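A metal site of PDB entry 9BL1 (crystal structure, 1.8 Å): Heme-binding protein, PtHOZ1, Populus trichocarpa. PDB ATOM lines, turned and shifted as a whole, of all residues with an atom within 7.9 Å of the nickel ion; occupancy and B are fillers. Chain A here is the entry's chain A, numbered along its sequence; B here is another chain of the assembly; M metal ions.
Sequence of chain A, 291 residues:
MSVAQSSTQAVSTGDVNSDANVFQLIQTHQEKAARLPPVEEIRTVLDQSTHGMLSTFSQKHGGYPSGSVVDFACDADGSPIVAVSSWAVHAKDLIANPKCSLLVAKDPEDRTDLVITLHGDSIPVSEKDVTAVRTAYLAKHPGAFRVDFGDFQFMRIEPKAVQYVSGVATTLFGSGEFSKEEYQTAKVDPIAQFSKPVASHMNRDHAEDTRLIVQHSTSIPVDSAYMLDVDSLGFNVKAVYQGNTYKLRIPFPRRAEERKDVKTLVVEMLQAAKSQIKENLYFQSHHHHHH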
ATOM      1  N   LYS A  60      18.878  -2.705 -23.138  1.00  0.00           N
ATOM      2  CA  LYS A  60      19.629  -1.808 -22.221  1.00  0.00           C
ATOM      3  C   LYS A  60      21.112  -1.786 -22.605  1.00  0.00           C
ATOM      4  O   LYS A  60      21.963  -1.502 -21.748  1.00  0.00           O
ATOM      5  CB  LYS A  60      19.383  -2.220 -20.752  1.00  0.00           C
ATOM      6  CG  LYS A  60      17.965  -1.952 -20.252  1.00  0.00           C
ATOM      7  CD  LYS A  60      17.683  -2.388 -18.785  1.00  0.00           C
ATOM      8  CE  LYS A  60      18.256  -3.744 -18.439  1.00  0.00           C
ATOM      9  NZ  LYS A  60      17.555  -4.415 -17.318  1.00  0.00           N
ATOM     10  N   HIS A  61      21.459  -2.022 -23.873  1.00  0.00           N
ATOM     11  CA  HIS A  61      22.854  -1.912 -24.303  1.00  0.00           C
ATOM     12  C   HIS A  61      22.877  -1.238 -25.686  1.00  0.00           C
ATOM     13  O   HIS A  61      23.789  -1.495 -26.439  1.00  0.00           O
ATOM     14  CB  HIS A  61      23.540  -3.273 -24.232  1.00  0.00           C
ATOM     15  CG  HIS A  61      25.015  -3.129 -24.274  1.00  0.00           C
ATOM     16  ND1 HIS A  61      25.717  -3.343 -25.435  1.00  0.00           N
ATOM     17  CD2 HIS A  61      25.913  -2.766 -23.331  1.00  0.00           C
ATOM     18  CE1 HIS A  61      27.012  -3.168 -25.199  1.00  0.00           C
ATOM     19  NE2 HIS A  61      27.185  -2.800 -23.903  1.00  0.00           N
ATOM     20  N   TYR A  64      23.496  -2.558 -29.413  1.00  0.00           N
ATOM     21  CA  TYR A  64      24.809  -3.125 -29.791  1.00  0.00           C
ATOM     22  C   TYR A  64      24.963  -4.555 -29.272  1.00  0.00           C
ATOM     23  O   TYR A  64      24.901  -4.787 -28.085  1.00  0.00           O
ATOM     24  CB  TYR A  64      25.965  -2.254 -29.304  1.00  0.00           C
ATOM     25  CG  TYR A  64      25.897  -0.872 -29.887  1.00  0.00           C
ATOM     26  CD1 TYR A  64      26.392  -0.592 -31.148  1.00  0.00           C
ATOM     27  CD2 TYR A  64      25.204   0.137 -29.228  1.00  0.00           C
ATOM     28  CE1 TYR A  64      26.297   0.683 -31.706  1.00  0.00           C
ATOM     29  CE2 TYR A  64      25.083   1.401 -29.776  1.00  0.00           C
ATOM     30  CZ  TYR A  64      25.582   1.668 -31.041  1.00  0.00           C
ATOM     31  OH  TYR A  64      25.418   2.909 -31.605  1.00  0.00           O
ATOM     32  N   PRO A  65      25.225  -5.546 -30.162  1.00  0.00           N
ATOM     33  CA  PRO A  65      25.643  -6.858 -29.729  1.00  0.00           C
ATOM     34  C   PRO A  65      27.078  -6.700 -29.213  1.00  0.00           C
ATOM     35  O   PRO A  65      27.783  -5.815 -29.659  1.00  0.00           O
ATOM     36  CB  PRO A  65      25.612  -7.748 -30.970  1.00  0.00           C
ATOM     37  CG  PRO A  65      25.816  -6.783 -32.085  1.00  0.00           C
ATOM     38  CD  PRO A  65      25.257  -5.445 -31.620  1.00  0.00           C
ATOM     39  N   SER A  66      27.464  -7.593 -28.304  1.00  0.00           N
ATOM     40  CA  SER A  66      28.700  -7.446 -27.516  1.00  0.00           C
ATOM     41  C   SER A  66      29.497  -8.744 -27.596  1.00  0.00           C
ATOM     42  O   SER A  66      28.912  -9.843 -27.710  1.00  0.00           O
ATOM     43  CB  SER A  66      28.361  -7.074 -26.085  1.00  0.00           C
ATOM     44  OG  SER A  66      27.779  -5.755 -26.023  1.00  0.00           O
ATOM     45  N   GLY A  67      30.814  -8.601 -27.486  1.00  0.00           N
ATOM     46  CA  GLY A  67      31.711  -9.738 -27.346  1.00  0.00           C
ATOM     47  C   GLY A  67      32.445  -9.733 -26.020  1.00  0.00           C
ATOM     48  O   GLY A  67      32.685  -8.674 -25.477  1.00  0.00           O
ATOM     49  N   VAL A  89      31.320  -7.862 -17.460  1.00  0.00           N
ATOM     50  CA  VAL A  89      30.831  -6.950 -18.524  1.00  0.00           C
ATOM     51  C   VAL A  89      30.593  -7.795 -19.780  1.00  0.00           C
ATOM     52  O   VAL A  89      31.482  -8.571 -20.195  1.00  0.00           O
ATOM     53  CB  VAL A  89      31.794  -5.792 -18.820  1.00  0.00           C
ATOM     54  CG1 VAL A  89      33.082  -6.291 -19.513  1.00  0.00           C
ATOM     55  CG2 VAL A  89      31.087  -4.745 -19.655  1.00  0.00           C
ATOM     56  N   HIS A  90      29.394  -7.644 -20.310  1.00  0.00           N
ATOM     57  CA  HIS A  90      28.857  -8.354 -21.482  1.00  0.00           C
ATOM     58  C   HIS A  90      28.525  -9.817 -21.155  1.00  0.00           C
ATOM     59  O   HIS A  90      27.396 -10.185 -21.431  1.00  0.00           O
ATOM     60  CB  HIS A  90      29.734  -8.124 -22.700  1.00  0.00           C
ATOM     61  CG  HIS A  90      29.947  -6.670 -22.959  1.00  0.00           C
ATOM     62  ND1 HIS A  90      31.211  -6.150 -23.121  1.00  0.00           N
ATOM     63  CD2 HIS A  90      29.097  -5.628 -23.019  1.00  0.00           C
ATOM     64  CE1 HIS A  90      31.123  -4.844 -23.306  1.00  0.00           C
ATOM     65  NE2 HIS A  90      29.846  -4.505 -23.253  1.00  0.00           N
ATOM     66  N   LYS A  92      27.763 -11.275 -18.573  1.00  0.00           N
ATOM     67  CA  LYS A  92      26.585 -11.318 -17.664  1.00  0.00           C
ATOM     68  C   LYS A  92      25.299 -11.371 -18.483  1.00  0.00           C
ATOM     69  O   LYS A  92      24.270 -11.837 -17.930  1.00  0.00           O
ATOM     70  CB  LYS A  92      26.575 -10.096 -16.740  1.00  0.00           C
ATOM     71  CG  LYS A  92      26.207  -8.806 -17.452  1.00  0.00           C
ATOM     72  CD  LYS A  92      26.076  -7.658 -16.501  1.00  0.00           C
ATOM     73  CE  LYS A  92      26.394  -6.300 -17.093  1.00  0.00           C
ATOM     74  NZ  LYS A  92      26.684  -5.344 -16.000  1.00  0.00           N
ATOM     75  N   ASP A  93      25.289 -10.873 -19.724  1.00  0.00           N
ATOM     76  CA  ASP A  93      24.094 -10.933 -20.609  1.00  0.00           C
ATOM     77  C   ASP A  93      23.498 -12.350 -20.672  1.00  0.00           C
ATOM     78  O   ASP A  93      22.310 -12.466 -20.924  1.00  0.00           O
ATOM     79  CB  ASP A  93      24.369 -10.489 -22.055  1.00  0.00           C
ATOM     80  CG  ASP A  93      24.812  -9.051 -22.273  1.00  0.00           C
ATOM     81  OD1 ASP A  93      24.647  -8.265 -21.347  1.00  0.00           O
ATOM     82  OD2 ASP A  93      25.321  -8.725 -23.422  1.00  0.00           O
ATOM     83  N   SER B 101      30.111  -4.787 -32.355  1.00  0.00           N
ATOM     84  CA  SER B 101      31.219  -4.608 -31.392  1.00  0.00           C
ATOM     85  C   SER B 101      32.475  -5.258 -31.972  1.00  0.00           C
ATOM     86  O   SER B 101      32.353  -6.256 -32.677  1.00  0.00           O
ATOM     87  CB  SER B 101      30.886  -5.207 -30.018  1.00  0.00           C
ATOM     88  OG  SER B 101      29.888  -4.425 -29.377  1.00  0.00           O
ATOM     89  N   THR B 117      36.964  -3.512 -25.895  1.00  0.00           N
ATOM     90  CA  THR B 117      35.679  -3.684 -26.601  1.00  0.00           C
ATOM     91  C   THR B 117      35.287  -2.309 -27.138  1.00  0.00           C
ATOM     92  O   THR B 117      35.318  -1.347 -26.349  1.00  0.00           O
ATOM     93  CB  THR B 117      34.636  -4.335 -25.688  1.00  0.00           C
ATOM     94  OG1 THR B 117      35.096  -5.650 -25.354  1.00  0.00           O
ATOM     95  CG2 THR B 117      33.290  -4.526 -26.362  1.00  0.00           C
ATOM     96  N   LEU B 118      35.018  -2.214 -28.433  1.00  0.00           N
ATOM     97  CA  LEU B 118      34.529  -0.957 -29.048  1.00  0.00           C
ATOM     98  C   LEU B 118      33.109  -1.279 -29.521  1.00  0.00           C
ATOM     99  O   LEU B 118      32.930  -2.214 -30.307  1.00  0.00           O
ATOM    100  CB  LEU B 118      35.524  -0.610 -30.166  1.00  0.00           C
ATOM    101  CG  LEU B 118      35.265   0.652 -30.982  1.00  0.00           C
ATOM    102  CD1 LEU B 118      36.595   1.179 -31.552  1.00  0.00           C
ATOM    103  CD2 LEU B 118      34.277   0.371 -32.098  1.00  0.00           C
ATOM    104  N   HIS B 119      32.120  -0.567 -29.015  1.00  0.00           N
ATOM    105  CA  HIS B 119      30.753  -0.616 -29.598  1.00  0.00           C
ATOM    106  C   HIS B 119      30.676   0.515 -30.640  1.00  0.00           C
ATOM    107  O   HIS B 119      31.088   1.689 -30.361  1.00  0.00           O
ATOM    108  CB  HIS B 119      29.674  -0.448 -28.539  1.00  0.00           C
ATOM    109  CG  HIS B 119      29.811  -1.320 -27.336  1.00  0.00           C
ATOM    110  ND1 HIS B 119      29.989  -2.679 -27.416  1.00  0.00           N
ATOM    111  CD2 HIS B 119      29.692  -1.028 -26.013  1.00  0.00           C
ATOM    112  CE1 HIS B 119      30.048  -3.191 -26.184  1.00  0.00           C
ATOM    113  NE2 HIS B 119      29.851  -2.182 -25.313  1.00  0.00           N
ATOM    114  N   ALA B 161      31.184   3.792 -27.923  1.00  0.00           N
ATOM    115  CA  ALA B 161      31.721   3.542 -26.575  1.00  0.00           C
ATOM    116  C   ALA B 161      32.945   2.643 -26.702  1.00  0.00           C
ATOM    117  O   ALA B 161      32.947   1.747 -27.573  1.00  0.00           O
ATOM    118  CB  ALA B 161      30.669   2.872 -25.733  1.00  0.00           C
ATOM    119  N   VAL B 162      33.942   2.871 -25.853  1.00  0.00           N
ATOM    120  CA  VAL B 162      35.140   1.992 -25.822  1.00  0.00           C
ATOM    121  C   VAL B 162      35.351   1.570 -24.369  1.00  0.00           C
ATOM    122  O   VAL B 162      35.279   2.422 -23.521  1.00  0.00           O
ATOM    123  CB  VAL B 162      36.386   2.678 -26.413  1.00  0.00           C
ATOM    124  CG1 VAL B 162      37.542   1.707 -26.497  1.00  0.00           C
ATOM    125  CG2 VAL B 162      36.107   3.261 -27.782  1.00  0.00           C
ATOM    126  N   GLN B 163      35.340   0.273 -24.106  1.00  0.00           N
ATOM    127  CA  GLN B 163      35.443  -0.311 -22.749  1.00  0.00           C
ATOM    128  C   GLN B 163      36.730  -1.134 -22.695  1.00  0.00           C
ATOM    129  O   GLN B 163      37.148  -1.623 -23.749  1.00  0.00           O
ATOM    130  CB  GLN B 163      34.232  -1.184 -22.438  1.00  0.00           C
ATOM    131  CG  GLN B 163      32.916  -0.425 -22.340  1.00  0.00           C
ATOM    132  CD  GLN B 163      31.706  -1.258 -21.983  1.00  0.00           C
ATOM    133  OE1 GLN B 163      31.254  -1.299 -20.833  1.00  0.00           O
ATOM    134  NE2 GLN B 163      31.063  -1.865 -22.969  1.00  0.00           N
ATOM    135  N   GLU B 177      35.984   2.951 -19.285  1.00  0.00           N
ATOM    136  CA  GLU B 177      35.243   3.210 -20.530  1.00  0.00           C
ATOM    137  C   GLU B 177      35.471   4.648 -20.972  1.00  0.00           C
ATOM    138  O   GLU B 177      35.700   5.547 -20.097  1.00  0.00           O
ATOM    139  CB  GLU B 177      33.771   2.842 -20.331  1.00  0.00           C
ATOM    140  CG  GLU B 177      33.055   3.649 -19.264  1.00  0.00           C
ATOM    141  CD  GLU B 177      33.356   3.196 -17.850  1.00  0.00           C
ATOM    142  OE1 GLU B 177      33.252   1.957 -17.588  1.00  0.00           O
ATOM    143  OE2 GLU B 177      33.772   4.065 -17.027  1.00  0.00           O
HETATM  144 NI    NI M   1      29.226  -2.458 -23.320  1.00  0.00          NI
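Four residues have an atom within 4 Å of the nickel ion: His 61, His 90, His 119 of chain B and Gln 163 of chain B.
ND1 of His 119 of chain B sits at hydrogen-bond distance from OG of Ser 101 of chain B. The backbone carbonyl oxygen of Thr 117 of chain B sits at hydrogen-bond distance from the backbone NH of Gln 163 of chain B. N of His 119 of chain B is in hydrogen-bond range of O of Ala 161 of chain B (2.8 Å). A ring nitrogen (ND1) of His 61 lies within hydrogen-bond range of the backbone carbonyl oxygen (O) of Tyr 64, 3.1 Å away. A ring nitrogen (ND1) of His 61 lies close to the side-chain hydroxyl (OG) of Ser 66 (3.2 Å).
The nickel ion is bound by the side-chain amide nitrogen of Gln 163 of chain B (2.0 Å), a ring nitrogen (NE2) of His 119 of chain B (2.1 Å), a ring nitrogen (NE2) of His 90 (2.1 Å) and a ring nitrogen (NE2) of His 61 (2.2 Å).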
